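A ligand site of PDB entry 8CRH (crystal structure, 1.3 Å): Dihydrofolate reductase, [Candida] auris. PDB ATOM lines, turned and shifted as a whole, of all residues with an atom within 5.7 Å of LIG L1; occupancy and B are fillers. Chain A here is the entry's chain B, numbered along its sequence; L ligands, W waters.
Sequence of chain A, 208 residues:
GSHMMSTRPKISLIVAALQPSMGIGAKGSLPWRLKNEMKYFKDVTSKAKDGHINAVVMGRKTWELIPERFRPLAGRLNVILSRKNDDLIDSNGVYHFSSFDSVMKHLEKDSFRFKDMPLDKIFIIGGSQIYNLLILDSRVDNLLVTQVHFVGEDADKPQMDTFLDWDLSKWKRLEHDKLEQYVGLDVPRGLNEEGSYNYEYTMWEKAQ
Water W1 lies within hydrogen-bond range of OG1 of Thr 146 (2.8 Å), O of Leu 144 (3.0 Å), O of Val 15 (3.2 Å) and N5 of LIG L1 (3.3 Å).
The backbone carbonyl oxygen (O) of Ile 125 lies within hydrogen-bond range of the side-chain hydroxyl (OH) of Tyr 131 (3.2 Å). The backbone NH (N) of Ile 14 lies within hydrogen-bond range of the backbone carbonyl oxygen (O) of Ile 124 (3.0 Å). OE1 of Glu 37 is in hydrogen-bond range of OG1 of Thr 146, 2.7 Å away. O of Ile 14 is in hydrogen-bond range of OH of Tyr 131, 2.6 Å away. The backbone NH (N) of Val 15 sits at hydrogen-bond distance from the backbone carbonyl oxygen (O) of Leu 144 (3.0 Å). O of Val 15 sits at hydrogen-bond distance from N of Thr 146, at 2.8 Å.
The side-chain hydroxyl of Tyr 131 is in hydrogen-bond range of a nitrogen (N4) of LIG L1 (3.3 Å). N of Ala 16 is in hydrogen-bond range of O14 of LG2 L2. N7 of LG2 L2 is in hydrogen-bond range of O of Ala 16 (2.9 Å). OE1 of Glu 37 lies within hydrogen-bond range of N5 of LIG L1, 2.7 Å away. O2 of LG2 L2 lies within hydrogen-bond range of N of Thr 62 (3.1 Å). An oxygen (O2) of LG2 L2 lies within hydrogen-bond range of the side-chain hydroxyl (OG1) of Thr 62, at 2.6 Å. The backbone carbonyl oxygen (O) of Ile 125 sits at hydrogen-bond distance from a nitrogen (N4) of LIG L1 (2.9 Å). The backbone carbonyl oxygen (O) of Ile 14 is in hydrogen-bond range of a nitrogen (N4) of LIG L1.
Val 15 touches LIG L1 (CA to N2, 3.4 Å). Ala 16 touches LIG L1 (N to N5, 3.7 Å). CD1 of Leu 30 touches C1 of LIG L1, at 3.8 Å. Met 38 touches LIG L1. Phe 41 touches LIG L1 (CZ to C6, 3.4 Å). CG2 of Thr 62 touches CL1 of LIG L1, at 3.6 Å. Ile 66 touches LIG L1. OG1 of Thr 146 touches N5 of LIG L1 (3.6 Å). Hydrophobic or aromatic side chains that line LIG L1: Ile 14, Ala 16, Leu 30, Met 38, Phe 41, Ile 66 and Ile 125. Of the 19 residues printed, 12 come within 4 Å of LIG L1.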
ATOM      1  N   ILE A  14      19.282 -28.211  -0.651  1.00  0.00           N
ATOM      2  CA  ILE A  14      18.788 -27.464   0.494  1.00  0.00           C
ATOM      3  C   ILE A  14      19.952 -27.198   1.449  1.00  0.00           C
ATOM      4  O   ILE A  14      20.674 -28.138   1.845  1.00  0.00           O
ATOM      5  CB  ILE A  14      17.595 -28.166   1.185  1.00  0.00           C
ATOM      6  CG1 ILE A  14      17.089 -27.349   2.363  1.00  0.00           C
ATOM      7  CG2 ILE A  14      17.932 -29.619   1.604  1.00  0.00           C
ATOM      8  CD1 ILE A  14      15.737 -27.822   2.873  1.00  0.00           C
ATOM      9  N   VAL A  15      20.136 -25.925   1.823  1.00  0.00           N
ATOM     10  CA  VAL A  15      21.323 -25.452   2.507  1.00  0.00           C
ATOM     11  C   VAL A  15      20.935 -24.216   3.312  1.00  0.00           C
ATOM     12  O   VAL A  15      19.981 -23.502   2.962  1.00  0.00           O
ATOM     13  CB  VAL A  15      22.432 -25.077   1.487  1.00  0.00           C
ATOM     14  CG1 VAL A  15      22.014 -23.878   0.598  1.00  0.00           C
ATOM     15  CG2 VAL A  15      23.789 -24.847   2.187  1.00  0.00           C
ATOM     16  N   ALA A  16      21.689 -23.956   4.378  1.00  0.00           N
ATOM     17  CA  ALA A  16      21.658 -22.676   5.093  1.00  0.00           C
ATOM     18  C   ALA A  16      23.033 -22.052   4.968  1.00  0.00           C
ATOM     19  O   ALA A  16      24.043 -22.679   5.311  1.00  0.00           O
ATOM     20  CB  ALA A  16      21.275 -22.869   6.564  1.00  0.00           C
ATOM     21  N   LEU A  30      27.668 -26.586  12.287  1.00  0.00           N
ATOM     22  CA  LEU A  30      27.146 -25.359  11.726  1.00  0.00           C
ATOM     23  C   LEU A  30      27.702 -24.169  12.507  1.00  0.00           C
ATOM     24  O   LEU A  30      28.000 -24.296  13.698  1.00  0.00           O
ATOM     25  CB  LEU A  30      25.616 -25.355  11.811  1.00  0.00           C
ATOM     26  CG  LEU A  30      24.931 -26.551  11.163  1.00  0.00           C
ATOM     27  CD1 LEU A  30      23.420 -26.437  11.348  1.00  0.00           C
ATOM     28  CD2 LEU A  30      25.291 -26.732   9.690  1.00  0.00           C
ATOM     29  N   TRP A  32      26.210 -21.526  13.479  1.00  0.00           N
ATOM     30  CA  TRP A  32      25.144 -20.889  14.254  1.00  0.00           C
ATOM     31  C   TRP A  32      24.273 -22.009  14.818  1.00  0.00           C
ATOM     32  O   TRP A  32      24.316 -23.148  14.357  1.00  0.00           O
ATOM     33  CB  TRP A  32      24.268 -19.988  13.374  1.00  0.00           C
ATOM     34  CG  TRP A  32      23.933 -20.664  12.066  1.00  0.00           C
ATOM     35  CD1 TRP A  32      22.965 -21.606  11.843  1.00  0.00           C
ATOM     36  CD2 TRP A  32      24.631 -20.509  10.839  1.00  0.00           C
ATOM     37  NE1 TRP A  32      22.997 -22.015  10.530  1.00  0.00           N
ATOM     38  CE2 TRP A  32      24.019 -21.359   9.897  1.00  0.00           C
ATOM     39  CE3 TRP A  32      25.718 -19.715  10.443  1.00  0.00           C
ATOM     40  CZ2 TRP A  32      24.457 -21.437   8.563  1.00  0.00           C
ATOM     41  CZ3 TRP A  32      26.145 -19.794   9.123  1.00  0.00           C
ATOM     42  CH2 TRP A  32      25.518 -20.657   8.212  1.00  0.00           C
ATOM     43  N   GLU A  37      15.314 -22.846  12.346  1.00  0.00           N
ATOM     44  CA  GLU A  37      15.833 -23.188  11.028  1.00  0.00           C
ATOM     45  C   GLU A  37      16.001 -24.701  10.897  1.00  0.00           C
ATOM     46  O   GLU A  37      15.643 -25.287   9.863  1.00  0.00           O
ATOM     47  CB  GLU A  37      17.165 -22.473  10.769  1.00  0.00           C
ATOM     48  CG  GLU A  37      17.475 -22.208   9.281  1.00  0.00           C
ATOM     49  CD  GLU A  37      17.787 -23.455   8.479  1.00  0.00           C
ATOM     50  OE1 GLU A  37      17.351 -23.558   7.313  1.00  0.00           O
ATOM     51  OE2 GLU A  37      18.499 -24.346   8.998  1.00  0.00           O
ATOM     52  N   MET A  38      16.516 -25.360  11.932  1.00  0.00           N
ATOM     53  CA  MET A  38      16.617 -26.809  11.878  1.00  0.00           C
ATOM     54  C   MET A  38      15.242 -27.455  11.776  1.00  0.00           C
ATOM     55  O   MET A  38      15.087 -28.468  11.080  1.00  0.00           O
ATOM     56  CB  MET A  38      17.428 -27.328  13.065  1.00  0.00           C
ATOM     57  CG  MET A  38      18.913 -26.940  12.937  1.00  0.00           C
ATOM     58  SD  MET A  38      19.891 -27.550  14.322  1.00  0.00           S
ATOM     59  CE  MET A  38      19.404 -26.400  15.595  1.00  0.00           C
ATOM     60  N   TYR A  40      12.647 -26.070  10.240  1.00  0.00           N
ATOM     61  CA  TYR A  40      12.295 -25.898   8.827  1.00  0.00           C
ATOM     62  C   TYR A  40      12.895 -27.015   7.966  1.00  0.00           C
ATOM     63  O   TYR A  40      12.199 -27.637   7.152  1.00  0.00           O
ATOM     64  CB  TYR A  40      12.766 -24.533   8.342  1.00  0.00           C
ATOM     65  CG  TYR A  40      12.641 -24.298   6.845  1.00  0.00           C
ATOM     66  CD1 TYR A  40      11.437 -23.827   6.290  1.00  0.00           C
ATOM     67  CD2 TYR A  40      13.728 -24.464   5.990  1.00  0.00           C
ATOM     68  CE1 TYR A  40      11.326 -23.569   4.927  1.00  0.00           C
ATOM     69  CE2 TYR A  40      13.633 -24.187   4.626  1.00  0.00           C
ATOM     70  CZ  TYR A  40      12.420 -23.745   4.099  1.00  0.00           C
ATOM     71  OH  TYR A  40      12.330 -23.451   2.726  1.00  0.00           O
ATOM     72  N   PHE A  41      14.198 -27.281   8.138  1.00  0.00           N
ATOM     73  CA  PHE A  41      14.829 -28.352   7.374  1.00  0.00           C
ATOM     74  C   PHE A  41      14.087 -29.669   7.594  1.00  0.00           C
ATOM     75  O   PHE A  41      13.791 -30.395   6.638  1.00  0.00           O
ATOM     76  CB  PHE A  41      16.282 -28.508   7.777  1.00  0.00           C
ATOM     77  CG  PHE A  41      16.902 -29.746   7.216  1.00  0.00           C
ATOM     78  CD1 PHE A  41      17.431 -29.755   5.926  1.00  0.00           C
ATOM     79  CD2 PHE A  41      16.905 -30.921   7.951  1.00  0.00           C
ATOM     80  CE1 PHE A  41      17.967 -30.920   5.406  1.00  0.00           C
ATOM     81  CE2 PHE A  41      17.419 -32.089   7.436  1.00  0.00           C
ATOM     82  CZ  PHE A  41      17.952 -32.085   6.150  1.00  0.00           C
ATOM     83  N   MET A  58      23.417 -37.182   1.019  1.00  0.00           N
ATOM     84  CA  MET A  58      24.438 -36.384   1.665  1.00  0.00           C
ATOM     85  C   MET A  58      25.804 -37.018   1.409  1.00  0.00           C
ATOM     86  O   MET A  58      25.903 -38.202   1.067  1.00  0.00           O
ATOM     87  CB  MET A  58      24.293 -36.355   3.193  1.00  0.00           C
ATOM     88  CG  MET A  58      24.302 -37.734   3.864  1.00  0.00           C
ATOM     89  SD  MET A  58      23.612 -37.708   5.518  1.00  0.00           S
ATOM     90  CE  MET A  58      21.919 -38.144   5.140  1.00  0.00           C
ATOM     91  N   THR A  62      29.239 -35.443   6.079  1.00  0.00           N
ATOM     92  CA  THR A  62      28.049 -34.924   6.749  1.00  0.00           C
ATOM     93  C   THR A  62      27.278 -36.044   7.448  1.00  0.00           C
ATOM     94  O   THR A  62      26.782 -35.860   8.562  1.00  0.00           O
ATOM     95  CB  THR A  62      27.211 -34.154   5.740  1.00  0.00           C
ATOM     96  OG1 THR A  62      27.935 -32.987   5.351  1.00  0.00           O
ATOM     97  CG2 THR A  62      25.872 -33.726   6.318  1.00  0.00           C
ATOM     98  N   ILE A  66      26.130 -36.546  11.851  1.00  0.00           N
ATOM     99  CA  ILE A  66      24.874 -36.845  12.552  1.00  0.00           C
ATOM    100  C   ILE A  66      25.193 -37.783  13.703  1.00  0.00           C
ATOM    101  O   ILE A  66      25.830 -38.823  13.480  1.00  0.00           O
ATOM    102  CB  ILE A  66      23.875 -37.487  11.605  1.00  0.00           C
ATOM    103  CG1 ILE A  66      23.666 -36.606  10.368  1.00  0.00           C
ATOM    104  CG2 ILE A  66      22.562 -37.795  12.364  1.00  0.00           C
ATOM    105  CD1 ILE A  66      22.978 -37.338   9.259  1.00  0.00           C
ATOM    106  N   LEU A  73      18.367 -40.435   9.376  1.00  0.00           N
ATOM    107  CA  LEU A  73      17.397 -39.391   9.685  1.00  0.00           C
ATOM    108  C   LEU A  73      15.986 -39.951   9.485  1.00  0.00           C
ATOM    109  O   LEU A  73      15.653 -40.452   8.403  1.00  0.00           O
ATOM    110  CB  LEU A  73      17.623 -38.194   8.773  1.00  0.00           C
ATOM    111  CG  LEU A  73      18.958 -37.463   8.960  1.00  0.00           C
ATOM    112  CD1 LEU A  73      19.024 -36.249   8.037  1.00  0.00           C
ATOM    113  CD2 LEU A  73      19.162 -37.020  10.396  1.00  0.00           C
ATOM    114  N   ILE A 124      19.198 -32.829  -1.704  1.00  0.00           N
ATOM    115  CA  ILE A 124      20.632 -32.920  -1.469  1.00  0.00           C
ATOM    116  C   ILE A 124      20.942 -32.009  -0.283  1.00  0.00           C
ATOM    117  O   ILE A 124      20.703 -30.804  -0.356  1.00  0.00           O
ATOM    118  CB  ILE A 124      21.442 -32.481  -2.701  1.00  0.00           C
ATOM    119  CG1 ILE A 124      21.025 -33.222  -3.976  1.00  0.00           C
ATOM    120  CG2 ILE A 124      22.947 -32.574  -2.430  1.00  0.00           C
ATOM    121  CD1 ILE A 124      21.023 -34.655  -3.889  1.00  0.00           C
ATOM    122  N   ILE A 125      21.436 -32.590   0.817  1.00  0.00           N
ATOM    123  CA  ILE A 125      21.467 -31.889   2.092  1.00  0.00           C
ATOM    124  C   ILE A 125      22.874 -31.505   2.545  1.00  0.00           C
ATOM    125  O   ILE A 125      23.049 -31.078   3.686  1.00  0.00           O
ATOM    126  CB  ILE A 125      20.705 -32.648   3.203  1.00  0.00           C
ATOM    127  CG1 ILE A 125      21.465 -33.928   3.626  1.00  0.00           C
ATOM    128  CG2 ILE A 125      19.275 -32.965   2.752  1.00  0.00           C
ATOM    129  CD1 ILE A 125      20.993 -34.525   4.945  1.00  0.00           C
ATOM    130  N   GLY A 126      23.883 -31.654   1.679  1.00  0.00           N
ATOM    131  CA  GLY A 126      25.245 -31.257   2.005  1.00  0.00           C
ATOM    132  C   GLY A 126      26.184 -32.451   2.065  1.00  0.00           C
ATOM    133  O   GLY A 126      25.770 -33.601   1.871  1.00  0.00           O
ATOM    134  N   TYR A 131      27.553 -30.416  -2.596  1.00  0.00           N
ATOM    135  CA  TYR A 131      26.871 -29.237  -3.135  1.00  0.00           C
ATOM    136  C   TYR A 131      27.614 -28.666  -4.337  1.00  0.00           C
ATOM    137  O   TYR A 131      26.995 -28.260  -5.329  1.00  0.00           O
ATOM    138  CB  TYR A 131      26.854 -28.140  -2.086  1.00  0.00           C
ATOM    139  CG  TYR A 131      25.851 -28.239  -0.964  1.00  0.00           C
ATOM    140  CD1 TYR A 131      24.534 -28.687  -1.167  1.00  0.00           C
ATOM    141  CD2 TYR A 131      26.210 -27.813   0.314  1.00  0.00           C
ATOM    142  CE1 TYR A 131      23.637 -28.716  -0.117  1.00  0.00           C
ATOM    143  CE2 TYR A 131      25.323 -27.841   1.350  1.00  0.00           C
ATOM    144  CZ  TYR A 131      24.038 -28.289   1.143  1.00  0.00           C
ATOM    145  OH  TYR A 131      23.216 -28.264   2.245  1.00  0.00           O
ATOM    146  N   LEU A 144      16.993 -24.548  -2.384  1.00  0.00           N
ATOM    147  CA  LEU A 144      16.281 -24.059  -1.223  1.00  0.00           C
ATOM    148  C   LEU A 144      17.354 -23.526  -0.284  1.00  0.00           C
ATOM    149  O   LEU A 144      18.045 -24.294   0.378  1.00  0.00           O
ATOM    150  CB  LEU A 144      15.460 -25.176  -0.587  1.00  0.00           C
ATOM    151  CG  LEU A 144      14.230 -25.626  -1.357  1.00  0.00           C
ATOM    152  CD1 LEU A 144      13.698 -26.944  -0.821  1.00  0.00           C
ATOM    153  CD2 LEU A 144      13.137 -24.560  -1.306  1.00  0.00           C
ATOM    154  N   THR A 146      18.433 -21.124   2.807  1.00  0.00           N
ATOM    155  CA  THR A 146      18.179 -20.231   3.937  1.00  0.00           C
ATOM    156  C   THR A 146      19.312 -19.236   3.964  1.00  0.00           C
ATOM    157  O   THR A 146      20.466 -19.619   4.206  1.00  0.00           O
ATOM    158  CB  THR A 146      18.120 -20.982   5.264  1.00  0.00           C
ATOM    159  OG1 THR A 146      17.096 -21.964   5.193  1.00  0.00           O
ATOM    160  CG2 THR A 146      17.773 -20.016   6.389  1.00  0.00           C
HETATM  161  C1  LIG L   1      21.583 -26.394   8.026  1.00  0.00           C
HETATM  162  C2  LIG L   1      20.336 -27.318   7.918  1.00  0.00           C
HETATM  163  C3  LIG L   1      19.224 -26.274   6.013  1.00  0.00           C
HETATM  164  C4  LIG L   1      20.545 -28.222   5.593  1.00  0.00           C
HETATM  165  C5  LIG L   1      21.530 -29.465   7.415  1.00  0.00           C
HETATM  166  C6  LIG L   1      20.708 -30.595   7.545  1.00  0.00           C
HETATM  167  C7  LIG L   1      21.184 -31.819   7.940  1.00  0.00           C
HETATM  168  C8  LIG L   1      22.539 -31.893   8.164  1.00  0.00           C
HETATM  169  C9  LIG L   1      23.383 -30.797   8.048  1.00  0.00           C
HETATM  170  C10 LIG L   1      22.878 -29.565   7.653  1.00  0.00           C
HETATM  171  C11 LIG L   1      19.925 -27.843   9.271  1.00  0.00           C
HETATM  172  N1  LIG L   1      19.385 -26.392   7.399  1.00  0.00           N
HETATM  173  N2  LIG L   1      19.788 -27.159   5.080  1.00  0.00           N
HETATM  174  N3  LIG L   1      20.792 -28.327   6.984  1.00  0.00           N
HETATM  175  N4  LIG L   1      21.064 -29.118   4.637  1.00  0.00           N
HETATM  176  N5  LIG L   1      18.374 -25.283   5.515  1.00  0.00           N
HETATM  177 CL1  LIG L   1      23.158 -33.484   8.655  1.00  0.00          CL
HETATM  178  P1  LG2 L   2      30.702 -33.638   2.529  1.00  0.00           P
HETATM  179  O1  LG2 L   2      30.577 -32.984   1.208  1.00  0.00           O
HETATM  180  O2  LG2 L   2      29.510 -33.841   3.411  1.00  0.00           O
HETATM  181  O3  LG2 L   2      31.336 -35.157   2.400  1.00  0.00           O
HETATM  182  C1  LG2 L   2      32.493 -35.147   1.580  1.00  0.00           C
HETATM  183  C2  LG2 L   2      32.675 -36.629   1.237  1.00  0.00           C
HETATM  184  O4  LG2 L   2      31.688 -36.968   0.287  1.00  0.00           O
HETATM  185  C3  LG2 L   2      34.044 -36.988   0.608  1.00  0.00           C
HETATM  186  O5  LG2 L   2      35.039 -37.171   1.583  1.00  0.00           O
HETATM  187  C4  LG2 L   2      33.648 -38.341  -0.061  1.00  0.00           C
HETATM  188  O6  LG2 L   2      33.477 -39.347   0.777  1.00  0.00           O
HETATM  189  C5  LG2 L   2      32.223 -37.982  -0.574  1.00  0.00           C
HETATM  190  N1  LG2 L   2      32.278 -37.468  -1.923  1.00  0.00           N
HETATM  191  C6  LG2 L   2      32.775 -36.230  -2.389  1.00  0.00           C
HETATM  192  N2  LG2 L   2      32.679 -36.101  -3.720  1.00  0.00           N
HETATM  193  C7  LG2 L   2      32.103 -37.328  -4.137  1.00  0.00           C
HETATM  194  C8  LG2 L   2      31.745 -37.824  -5.390  1.00  0.00           C
HETATM  195  N3  LG2 L   2      31.944 -37.078  -6.526  1.00  0.00           N
HETATM  196  N4  LG2 L   2      31.190 -39.067  -5.529  1.00  0.00           N
HETATM  197  C9  LG2 L   2      31.025 -39.765  -4.353  1.00  0.00           C
HETATM  198  N5  LG2 L   2      31.317 -39.427  -3.100  1.00  0.00           N
HETATM  199  C10 LG2 L   2      31.856 -38.177  -3.020  1.00  0.00           C
HETATM  200  O7  LG2 L   2      31.914 -32.944   3.468  1.00  0.00           O
HETATM  201  P2  LG2 L   2      32.328 -31.405   3.491  1.00  0.00           P
HETATM  202  O8  LG2 L   2      33.493 -31.360   4.392  1.00  0.00           O
HETATM  203  O9  LG2 L   2      32.388 -30.725   2.145  1.00  0.00           O
HETATM  204  O10 LG2 L   2      31.042 -30.589   4.300  1.00  0.00           O
HETATM  205  C11 LG2 L   2      30.996 -30.774   5.689  1.00  0.00           C
HETATM  206  C12 LG2 L   2      30.797 -29.361   6.321  1.00  0.00           C
HETATM  207  O11 LG2 L   2      29.609 -28.759   5.775  1.00  0.00           O
HETATM  208  C13 LG2 L   2      30.626 -29.389   7.859  1.00  0.00           C
HETATM  209  O12 LG2 L   2      31.145 -28.169   8.379  1.00  0.00           O
HETATM  210  C14 LG2 L   2      29.128 -29.377   8.017  1.00  0.00           C
HETATM  211  O13 LG2 L   2      28.726 -28.815   9.238  1.00  0.00           O
HETATM  212  C15 LG2 L   2      28.757 -28.405   6.854  1.00  0.00           C
HETATM  213  N6  LG2 L   2      27.356 -28.544   6.419  1.00  0.00           N
HETATM  214  C16 LG2 L   2      26.544 -27.412   6.399  1.00  0.00           C
HETATM  215  C17 LG2 L   2      25.317 -27.466   5.806  1.00  0.00           C
HETATM  216  C18 LG2 L   2      24.498 -26.248   5.788  1.00  0.00           C
HETATM  217  O14 LG2 L   2      23.452 -26.178   5.152  1.00  0.00           O
HETATM  218  N7  LG2 L   2      24.917 -25.142   6.494  1.00  0.00           N
HETATM  219  C19 LG2 L   2      24.790 -28.688   5.153  1.00  0.00           C
HETATM  220  C20 LG2 L   2      25.640 -29.887   5.408  1.00  0.00           C
HETATM  221  C21 LG2 L   2      26.847 -29.795   5.995  1.00  0.00           C
HETATM  222  P3  LG2 L   2      34.840 -40.482   0.787  1.00  0.00           P
HETATM  223  O15 LG2 L   2      34.827 -40.877  -0.653  1.00  0.00           O
HETATM  224  O16 LG2 L   2      36.012 -39.603   1.257  1.00  0.00           O
HETATM  225  O17 LG2 L   2      34.297 -41.465   1.784  1.00  0.00           O
HETATM  226  C1  LG3 L   3      20.584 -33.669  11.360  1.00  0.00           C
HETATM  227  C2  LG3 L   3      20.462 -33.166  12.794  1.00  0.00           C
HETATM  228  C3  LG3 L   3      19.802 -34.432  14.866  1.00  0.00           C
HETATM  229  C4  LG3 L   3      22.046 -33.380  14.736  1.00  0.00           C
HETATM  230  C5  LG3 L   3      22.833 -32.175  12.726  1.00  0.00           C
HETATM  231  C6  LG3 L   3      22.978 -30.809  12.805  1.00  0.00           C
HETATM  232  C7  LG3 L   3      24.038 -30.208  12.139  1.00  0.00           C
HETATM  233  C8  LG3 L   3      24.939 -30.981  11.434  1.00  0.00           C
HETATM  234  C9  LG3 L   3      24.812 -32.356  11.370  1.00  0.00           C
HETATM  235  C10 LG3 L   3      23.757 -32.941  12.026  1.00  0.00           C
HETATM  236  C11 LG3 L   3      19.746 -31.822  12.946  1.00  0.00           C
HETATM  237  N1  LG3 L   3      19.514 -33.987  13.528  1.00  0.00           N
HETATM  238  N2  LG3 L   3      21.077 -34.130  15.481  1.00  0.00           N
HETATM  239  N3  LG3 L   3      21.765 -32.914  13.398  1.00  0.00           N
HETATM  240  N4  LG3 L   3      23.334 -33.074  15.324  1.00  0.00           N
HETATM  241  N5  LG3 L   3      18.818 -35.196  15.620  1.00  0.00           N
HETATM  242 CL1  LG3 L   3      26.300 -30.215  10.587  1.00  0.00          CL
HETATM  243  O   HOH W   1      16.765 -23.768   3.047  1.00  0.00           O
